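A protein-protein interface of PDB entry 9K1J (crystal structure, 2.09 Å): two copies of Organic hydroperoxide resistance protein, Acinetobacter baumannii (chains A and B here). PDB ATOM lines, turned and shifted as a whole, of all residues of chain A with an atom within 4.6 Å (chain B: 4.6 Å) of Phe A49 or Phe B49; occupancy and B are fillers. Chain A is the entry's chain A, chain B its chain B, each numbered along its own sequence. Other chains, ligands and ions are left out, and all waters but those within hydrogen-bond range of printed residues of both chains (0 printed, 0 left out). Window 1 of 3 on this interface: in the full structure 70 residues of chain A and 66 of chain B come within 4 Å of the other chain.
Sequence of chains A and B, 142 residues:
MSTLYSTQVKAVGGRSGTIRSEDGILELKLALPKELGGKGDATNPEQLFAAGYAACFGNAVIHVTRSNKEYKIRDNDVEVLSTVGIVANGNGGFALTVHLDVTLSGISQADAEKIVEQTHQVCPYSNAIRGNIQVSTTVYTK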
ATOM      1  N   PRO A  45      24.933 -33.151  10.280  1.00  0.00           N
ATOM      2  CA  PRO A  45      23.798 -32.205  10.161  1.00  0.00           C
ATOM      3  C   PRO A  45      23.714 -31.458   8.841  1.00  0.00           C
ATOM      4  O   PRO A  45      22.614 -31.277   8.308  1.00  0.00           O
ATOM      5  CB  PRO A  45      24.038 -31.246  11.332  1.00  0.00           C
ATOM      6  CG  PRO A  45      24.581 -32.198  12.412  1.00  0.00           C
ATOM      7  CD  PRO A  45      25.535 -33.116  11.632  1.00  0.00           C
ATOM      8  N   GLU A  46      24.846 -31.015   8.302  1.00  0.00           N
ATOM      9  CA  GLU A  46      24.811 -30.279   7.042  1.00  0.00           C
ATOM     10  C   GLU A  46      24.329 -31.150   5.897  1.00  0.00           C
ATOM     11  O   GLU A  46      23.572 -30.689   5.061  1.00  0.00           O
ATOM     12  CB  GLU A  46      26.190 -29.692   6.736  1.00  0.00           C
ATOM     13  CG  GLU A  46      26.518 -28.537   7.643  1.00  0.00           C
ATOM     14  CD  GLU A  46      26.767 -28.991   9.078  1.00  0.00           C
ATOM     15  OE1 GLU A  46      27.499 -29.995   9.270  1.00  0.00           O
ATOM     16  OE2 GLU A  46      26.206 -28.361  10.011  1.00  0.00           O
ATOM     17  N   GLN A  47      24.747 -32.415   5.847  1.00  0.00           N
ATOM     18  CA  GLN A  47      24.275 -33.313   4.795  1.00  0.00           C
ATOM     19  C   GLN A  47      22.790 -33.613   4.931  1.00  0.00           C
ATOM     20  O   GLN A  47      22.070 -33.696   3.927  1.00  0.00           O
ATOM     21  CB  GLN A  47      25.060 -34.633   4.818  1.00  0.00           C
ATOM     22  CG  GLN A  47      26.386 -34.548   4.108  1.00  0.00           C
ATOM     23  CD  GLN A  47      27.047 -35.909   3.913  1.00  0.00           C
ATOM     24  OE1 GLN A  47      26.602 -36.929   4.468  1.00  0.00           O
ATOM     25  NE2 GLN A  47      28.103 -35.932   3.091  1.00  0.00           N
ATOM     26  N   LEU A  48      22.319 -33.815   6.166  1.00  0.00           N
ATOM     27  CA  LEU A  48      20.903 -34.085   6.385  1.00  0.00           C
ATOM     28  C   LEU A  48      20.059 -32.885   5.955  1.00  0.00           C
ATOM     29  O   LEU A  48      19.011 -33.043   5.311  1.00  0.00           O
ATOM     30  CB  LEU A  48      20.675 -34.431   7.868  1.00  0.00           C
ATOM     31  CG  LEU A  48      21.269 -35.760   8.322  1.00  0.00           C
ATOM     32  CD1 LEU A  48      21.307 -35.930   9.877  1.00  0.00           C
ATOM     33  CD2 LEU A  48      20.471 -36.880   7.705  1.00  0.00           C
ATOM     34  N   PHE A  49      20.538 -31.676   6.263  1.00  0.00           N
ATOM     35  CA  PHE A  49      19.836 -30.459   5.864  1.00  0.00           C
ATOM     36  C   PHE A  49      19.873 -30.271   4.351  1.00  0.00           C
ATOM     37  O   PHE A  49      18.849 -29.963   3.729  1.00  0.00           O
ATOM     38  CB  PHE A  49      20.464 -29.244   6.554  1.00  0.00           C
ATOM     39  CG  PHE A  49      19.731 -27.969   6.269  1.00  0.00           C
ATOM     40  CD1 PHE A  49      18.545 -27.683   6.928  1.00  0.00           C
ATOM     41  CD2 PHE A  49      20.193 -27.079   5.308  1.00  0.00           C
ATOM     42  CE1 PHE A  49      17.835 -26.499   6.646  1.00  0.00           C
ATOM     43  CE2 PHE A  49      19.501 -25.900   5.022  1.00  0.00           C
ATOM     44  CZ  PHE A  49      18.316 -25.611   5.691  1.00  0.00           C
ATOM     45  N   ALA A  50      21.063 -30.399   3.750  1.00  0.00           N
ATOM     46  CA  ALA A  50      21.183 -30.341   2.294  1.00  0.00           C
ATOM     47  C   ALA A  50      20.193 -31.290   1.625  1.00  0.00           C
ATOM     48  O   ALA A  50      19.540 -30.923   0.639  1.00  0.00           O
ATOM     49  CB  ALA A  50      22.618 -30.683   1.873  1.00  0.00           C
ATOM     50  N   ALA A  51      20.039 -32.506   2.174  1.00  0.00           N
ATOM     51  CA  ALA A  51      19.141 -33.495   1.581  1.00  0.00           C
ATOM     52  C   ALA A  51      17.670 -33.108   1.746  1.00  0.00           C
ATOM     53  O   ALA A  51      16.881 -33.192   0.791  1.00  0.00           O
ATOM     54  CB  ALA A  51      19.387 -34.861   2.222  1.00  0.00           C
ATOM     55  N   GLY A  52      17.266 -32.760   2.975  1.00  0.00           N
ATOM     56  CA  GLY A  52      15.898 -32.314   3.190  1.00  0.00           C
ATOM     57  C   GLY A  52      15.521 -31.154   2.288  1.00  0.00           C
ATOM     58  O   GLY A  52      14.444 -31.135   1.672  1.00  0.00           O
ATOM     59  N   TYR A  53      16.418 -30.190   2.149  1.00  0.00           N
ATOM     60  CA  TYR A  53      16.068 -29.007   1.367  1.00  0.00           C
ATOM     61  C   TYR A  53      16.107 -29.273  -0.134  1.00  0.00           C
ATOM     62  O   TYR A  53      15.185 -28.872  -0.856  1.00  0.00           O
ATOM     63  CB  TYR A  53      16.920 -27.829   1.833  1.00  0.00           C
ATOM     64  CG  TYR A  53      16.766 -26.486   1.142  1.00  0.00           C
ATOM     65  CD1 TYR A  53      15.519 -26.019   0.775  1.00  0.00           C
ATOM     66  CD2 TYR A  53      17.739 -25.522   1.357  1.00  0.00           C
ATOM     67  CE1 TYR A  53      15.331 -24.729   0.284  1.00  0.00           C
ATOM     68  CE2 TYR A  53      17.570 -24.205   0.909  1.00  0.00           C
ATOM     69  CZ  TYR A  53      16.352 -23.817   0.381  1.00  0.00           C
ATOM     70  OH  TYR A  53      16.134 -22.537  -0.053  1.00  0.00           O
ATOM     71  N   VAL A  84      25.661 -27.147   0.975  1.00  0.00           N
ATOM     72  CA  VAL A  84      25.450 -26.551   2.289  1.00  0.00           C
ATOM     73  C   VAL A  84      26.789 -26.501   3.007  1.00  0.00           C
ATOM     74  O   VAL A  84      27.497 -27.513   3.085  1.00  0.00           O
ATOM     75  CB  VAL A  84      24.410 -27.327   3.121  1.00  0.00           C
ATOM     76  CG1 VAL A  84      24.383 -26.782   4.556  1.00  0.00           C
ATOM     77  CG2 VAL A  84      23.015 -27.231   2.490  1.00  0.00           C
ATOM     78  N   LEU A  96      24.752 -21.368   8.447  1.00  0.00           N
ATOM     79  CA  LEU A  96      24.808 -22.164   7.233  1.00  0.00           C
ATOM     80  C   LEU A  96      24.880 -21.250   6.018  1.00  0.00           C
ATOM     81  O   LEU A  96      24.370 -20.127   6.035  1.00  0.00           O
ATOM     82  CB  LEU A  96      23.586 -23.071   7.122  1.00  0.00           C
ATOM     83  CG  LEU A  96      23.420 -24.055   8.279  1.00  0.00           C
ATOM     84  CD1 LEU A  96      22.186 -24.869   8.038  1.00  0.00           C
ATOM     85  CD2 LEU A  96      24.641 -24.987   8.436  1.00  0.00           C
ATOM     86  N   VAL A  98      23.957 -21.789   1.753  1.00  0.00           N
ATOM     87  CA  VAL A  98      23.221 -22.700   0.878  1.00  0.00           C
ATOM     88  C   VAL A  98      23.328 -22.226  -0.573  1.00  0.00           C
ATOM     89  O   VAL A  98      23.105 -21.047  -0.874  1.00  0.00           O
ATOM     90  CB  VAL A  98      21.733 -22.841   1.258  1.00  0.00           C
ATOM     91  CG1 VAL A  98      21.093 -23.897   0.360  1.00  0.00           C
ATOM     92  CG2 VAL A  98      21.516 -23.177   2.758  1.00  0.00           C
ATOM     93  N   TYR A 125      11.180 -24.644   3.167  1.00  0.00           N
ATOM     94  CA  TYR A 125      12.537 -24.460   3.669  1.00  0.00           C
ATOM     95  C   TYR A 125      13.093 -23.112   3.224  1.00  0.00           C
ATOM     96  O   TYR A 125      13.694 -22.378   4.016  1.00  0.00           O
ATOM     97  CB  TYR A 125      13.422 -25.629   3.203  1.00  0.00           C
ATOM     98  CG  TYR A 125      13.003 -26.945   3.823  1.00  0.00           C
ATOM     99  CD1 TYR A 125      11.728 -27.461   3.598  1.00  0.00           C
ATOM    100  CD2 TYR A 125      13.880 -27.677   4.614  1.00  0.00           C
ATOM    101  CE1 TYR A 125      11.326 -28.635   4.160  1.00  0.00           C
ATOM    102  CE2 TYR A 125      13.488 -28.864   5.178  1.00  0.00           C
ATOM    103  CZ  TYR A 125      12.207 -29.335   4.948  1.00  0.00           C
ATOM    104  OH  TYR A 125      11.797 -30.514   5.502  1.00  0.00           O
ATOM    105  N   ILE A 129      14.297 -19.892   5.956  1.00  0.00           N
ATOM    106  CA  ILE A 129      15.608 -19.279   6.158  1.00  0.00           C
ATOM    107  C   ILE A 129      15.708 -17.850   5.623  1.00  0.00           C
ATOM    108  O   ILE A 129      16.760 -17.223   5.797  1.00  0.00           O
ATOM    109  CB  ILE A 129      16.739 -20.149   5.568  1.00  0.00           C
ATOM    110  CG1 ILE A 129      16.644 -20.233   4.050  1.00  0.00           C
ATOM    111  CG2 ILE A 129      16.733 -21.553   6.176  1.00  0.00           C
ATOM    112  CD1 ILE A 129      17.630 -21.336   3.486  1.00  0.00           C
ATOM    113  N   PRO B  45      11.516 -35.042   3.906  1.00  0.00           N
ATOM    114  CA  PRO B  45      12.254 -33.813   4.239  1.00  0.00           C
ATOM    115  C   PRO B  45      12.106 -33.333   5.677  1.00  0.00           C
ATOM    116  O   PRO B  45      13.045 -32.720   6.221  1.00  0.00           O
ATOM    117  CB  PRO B  45      11.651 -32.802   3.253  1.00  0.00           C
ATOM    118  CG  PRO B  45      11.419 -33.653   2.033  1.00  0.00           C
ATOM    119  CD  PRO B  45      10.744 -34.861   2.660  1.00  0.00           C
ATOM    120  N   GLU B  46      10.938 -33.535   6.295  1.00  0.00           N
ATOM    121  CA  GLU B  46      10.737 -33.069   7.671  1.00  0.00           C
ATOM    122  C   GLU B  46      11.519 -33.928   8.648  1.00  0.00           C
ATOM    123  O   GLU B  46      12.150 -33.411   9.569  1.00  0.00           O
ATOM    124  CB  GLU B  46       9.249 -33.062   8.026  1.00  0.00           C
ATOM    125  CG  GLU B  46       8.484 -31.928   7.337  1.00  0.00           C
ATOM    126  CD  GLU B  46       8.381 -32.146   5.836  1.00  0.00           C
ATOM    127  OE1 GLU B  46       7.979 -33.270   5.422  1.00  0.00           O
ATOM    128  OE2 GLU B  46       8.764 -31.219   5.073  1.00  0.00           O
ATOM    129  N   GLN B  47      11.529 -35.240   8.423  1.00  0.00           N
ATOM    130  CA  GLN B  47      12.322 -36.159   9.235  1.00  0.00           C
ATOM    131  C   GLN B  47      13.828 -35.888   9.097  1.00  0.00           C
ATOM    132  O   GLN B  47      14.579 -35.917  10.084  1.00  0.00           O
ATOM    133  CB  GLN B  47      11.944 -37.575   8.788  1.00  0.00           C
ATOM    134  CG  GLN B  47      12.112 -38.670   9.768  1.00  0.00           C
ATOM    135  CD  GLN B  47      11.463 -39.941   9.254  1.00  0.00           C
ATOM    136  OE1 GLN B  47      12.036 -40.648   8.426  1.00  0.00           O
ATOM    137  NE2 GLN B  47      10.244 -40.219   9.724  1.00  0.00           N
ATOM    138  N   LEU B  48      14.282 -35.570   7.886  1.00  0.00           N
ATOM    139  CA  LEU B  48      15.695 -35.254   7.684  1.00  0.00           C
ATOM    140  C   LEU B  48      16.070 -33.920   8.331  1.00  0.00           C
ATOM    141  O   LEU B  48      17.121 -33.817   8.985  1.00  0.00           O
ATOM    142  CB  LEU B  48      16.018 -35.229   6.188  1.00  0.00           C
ATOM    143  CG  LEU B  48      16.131 -36.563   5.445  1.00  0.00           C
ATOM    144  CD1 LEU B  48      16.061 -36.290   3.944  1.00  0.00           C
ATOM    145  CD2 LEU B  48      17.407 -37.349   5.828  1.00  0.00           C
ATOM    146  N   PHE B  49      15.233 -32.886   8.159  1.00  0.00           N
ATOM    147  CA  PHE B  49      15.435 -31.626   8.891  1.00  0.00           C
ATOM    148  C   PHE B  49      15.435 -31.843  10.410  1.00  0.00           C
ATOM    149  O   PHE B  49      16.302 -31.318  11.128  1.00  0.00           O
ATOM    150  CB  PHE B  49      14.350 -30.624   8.500  1.00  0.00           C
ATOM    151  CG  PHE B  49      14.480 -29.254   9.194  1.00  0.00           C
ATOM    152  CD1 PHE B  49      15.609 -28.475   9.037  1.00  0.00           C
ATOM    153  CD2 PHE B  49      13.452 -28.748   9.971  1.00  0.00           C
ATOM    154  CE1 PHE B  49      15.723 -27.233   9.661  1.00  0.00           C
ATOM    155  CE2 PHE B  49      13.575 -27.495  10.613  1.00  0.00           C
ATOM    156  CZ  PHE B  49      14.711 -26.749  10.449  1.00  0.00           C
ATOM    157  N   ALA B  50      14.450 -32.595  10.923  1.00  0.00           N
ATOM    158  CA  ALA B  50      14.368 -32.835  12.363  1.00  0.00           C
ATOM    159  C   ALA B  50      15.646 -33.482  12.874  1.00  0.00           C
ATOM    160  O   ALA B  50      16.175 -33.093  13.924  1.00  0.00           O
ATOM    161  CB  ALA B  50      13.165 -33.731  12.685  1.00  0.00           C
ATOM    162  N   ALA B  51      16.163 -34.466  12.129  1.00  0.00           N
ATOM    163  CA  ALA B  51      17.360 -35.178  12.554  1.00  0.00           C
ATOM    164  C   ALA B  51      18.568 -34.253  12.567  1.00  0.00           C
ATOM    165  O   ALA B  51      19.341 -34.229  13.539  1.00  0.00           O
ATOM    166  CB  ALA B  51      17.600 -36.370  11.619  1.00  0.00           C
ATOM    167  N   GLY B  52      18.746 -33.475  11.490  1.00  0.00           N
ATOM    168  CA  GLY B  52      19.902 -32.595  11.439  1.00  0.00           C
ATOM    169  C   GLY B  52      19.851 -31.554  12.541  1.00  0.00           C
ATOM    170  O   GLY B  52      20.863 -31.242  13.184  1.00  0.00           O
ATOM    171  N   TYR B  53      18.664 -31.041  12.825  1.00  0.00           N
ATOM    172  CA  TYR B  53      18.597 -29.996  13.839  1.00  0.00           C
ATOM    173  C   TYR B  53      18.710 -30.533  15.247  1.00  0.00           C
ATOM    174  O   TYR B  53      19.424 -29.944  16.066  1.00  0.00           O
ATOM    175  CB  TYR B  53      17.402 -29.088  13.558  1.00  0.00           C
ATOM    176  CG  TYR B  53      17.069 -27.981  14.541  1.00  0.00           C
ATOM    177  CD1 TYR B  53      18.035 -27.134  14.979  1.00  0.00           C
ATOM    178  CD2 TYR B  53      15.819 -27.404  14.435  1.00  0.00           C
ATOM    179  CE1 TYR B  53      17.723 -25.998  15.742  1.00  0.00           C
ATOM    180  CE2 TYR B  53      15.477 -26.209  15.104  1.00  0.00           C
ATOM    181  CZ  TYR B  53      16.451 -25.499  15.757  1.00  0.00           C
ATOM    182  OH  TYR B  53      16.179 -24.312  16.456  1.00  0.00           O
ATOM    183  N   VAL B  84       9.023 -31.879  14.223  1.00  0.00           N
ATOM    184  CA  VAL B  84       8.889 -31.004  13.068  1.00  0.00           C
ATOM    185  C   VAL B  84       7.559 -31.311  12.411  1.00  0.00           C
ATOM    186  O   VAL B  84       7.217 -32.482  12.213  1.00  0.00           O
ATOM    187  CB  VAL B  84      10.057 -31.174  12.095  1.00  0.00           C
ATOM    188  CG1 VAL B  84       9.783 -30.412  10.806  1.00  0.00           C
ATOM    189  CG2 VAL B  84      11.345 -30.696  12.770  1.00  0.00           C
ATOM    190  N   LEU B  96       6.824 -24.717   8.088  1.00  0.00           N
ATOM    191  CA  LEU B  96       7.354 -25.683   9.038  1.00  0.00           C
ATOM    192  C   LEU B  96       7.138 -25.174  10.459  1.00  0.00           C
ATOM    193  O   LEU B  96       7.147 -23.971  10.707  1.00  0.00           O
ATOM    194  CB  LEU B  96       8.850 -25.911   8.806  1.00  0.00           C
ATOM    195  CG  LEU B  96       9.242 -26.575   7.477  1.00  0.00           C
ATOM    196  CD1 LEU B  96      10.749 -26.546   7.322  1.00  0.00           C
ATOM    197  CD2 LEU B  96       8.725 -28.018   7.446  1.00  0.00           C
ATOM    198  N   VAL B  98       8.623 -26.246  14.564  1.00  0.00           N
ATOM    199  CA  VAL B  98       9.658 -26.988  15.270  1.00  0.00           C
ATOM    200  C   VAL B  98       9.459 -26.814  16.772  1.00  0.00           C
ATOM    201  O   VAL B  98       9.354 -25.690  17.269  1.00  0.00           O
ATOM    202  CB  VAL B  98      11.080 -26.525  14.882  1.00  0.00           C
ATOM    203  CG1 VAL B  98      12.099 -27.356  15.652  1.00  0.00           C
ATOM    204  CG2 VAL B  98      11.304 -26.622  13.371  1.00  0.00           C
ATOM    205  N   TYR B 125      21.356 -23.954  12.806  1.00  0.00           N
ATOM    206  CA  TYR B 125      19.952 -24.112  12.414  1.00  0.00           C
ATOM    207  C   TYR B 125      19.048 -23.108  13.125  1.00  0.00           C
ATOM    208  O   TYR B 125      18.124 -22.555  12.514  1.00  0.00           O
ATOM    209  CB  TYR B 125      19.463 -25.498  12.756  1.00  0.00           C
ATOM    210  CG  TYR B 125      19.934 -26.614  11.902  1.00  0.00           C
ATOM    211  CD1 TYR B 125      21.277 -26.947  11.806  1.00  0.00           C
ATOM    212  CD2 TYR B 125      18.994 -27.418  11.272  1.00  0.00           C
ATOM    213  CE1 TYR B 125      21.667 -28.032  11.033  1.00  0.00           C
ATOM    214  CE2 TYR B 125      19.349 -28.501  10.532  1.00  0.00           C
ATOM    215  CZ  TYR B 125      20.679 -28.813  10.396  1.00  0.00           C
ATOM    216  OH  TYR B 125      20.969 -29.926   9.620  1.00  0.00           O
ATOM    217  N   ILE B 129      16.788 -20.158  11.094  1.00  0.00           N
ATOM    218  CA  ILE B 129      15.328 -20.057  11.000  1.00  0.00           C
ATOM    219  C   ILE B 129      14.731 -18.977  11.916  1.00  0.00           C
ATOM    220  O   ILE B 129      13.502 -18.862  12.004  1.00  0.00           O
ATOM    221  CB  ILE B 129      14.697 -21.425  11.283  1.00  0.00           C
ATOM    222  CG1 ILE B 129      14.948 -21.806  12.736  1.00  0.00           C
ATOM    223  CG2 ILE B 129      15.329 -22.491  10.403  1.00  0.00           C
ATOM    224  CD1 ILE B 129      14.480 -23.208  13.046  1.00  0.00           C
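OH of Tyr A125 lies within hydrogen-bond range of O of Pro B45, at 2.6 Å.
OH of Tyr A125 is in hydrogen-bond range of OE2 of Glu B46.
OH of Tyr B125 sits at hydrogen-bond distance from O of Pro A45 (2.5 Å).
Among the printed residues, pairs that only touch across the chains: Phe A49 with Tyr B125, Gly A52 with Pro B45, Leu A48 with Leu B48, Pro A45 with Gly B52, Phe A49 with Phe B49, Tyr A125 with Leu B96, Gly A52 with Leu B48, Tyr A125 with Phe B49 and Leu A48 with Gly B52.
Phe A49 touches two residues of chain B.
Of the printed residues of chain A, Pro B45 touches Gly A52 (3.6 Å) and Tyr A125 (2.6 Å).
Printed residues of chain A within 4 Å of Glu B46: Tyr A125 (3.1 Å).
Phe B49 touches two residues of chain A.
Of the 14 printed residues of chain A, 5 touch a printed residue of chain B.
Hydrophobic or aromatic side chains of chain A within 4 Å of the printed part of chain B: Pro A45, Leu A48, Phe A49 and Tyr A125.
Hydrophobic or aromatic side chains of chain B within 4 Å of the printed part of chain A: Pro B45, Leu B48, Phe B49, Leu B96 and Tyr B125.
Among the printed residues, no Asp or Glu carboxylate lies within 4 Å of a Lys or Arg side-chain nitrogen of the other chain.
Pro A45 touches Tyr B125, and with the chains exchanged Tyr A125 touches Pro B45.
Leu A48 touches Gly B52, and with the chains exchanged Gly A52 touches Leu B48.
Phe A49 touches Tyr B125, and with the chains exchanged Tyr A125 touches Phe B49.
Tyr A125 touches Glu B46, but with the chains exchanged Glu A46 does not touch Tyr B125 (4.2 Å).
Positions printed for both chains: 45, 46, 47, 48, 49, 50, 51, 52, 53, 84, 96, 98, 125 and 129.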
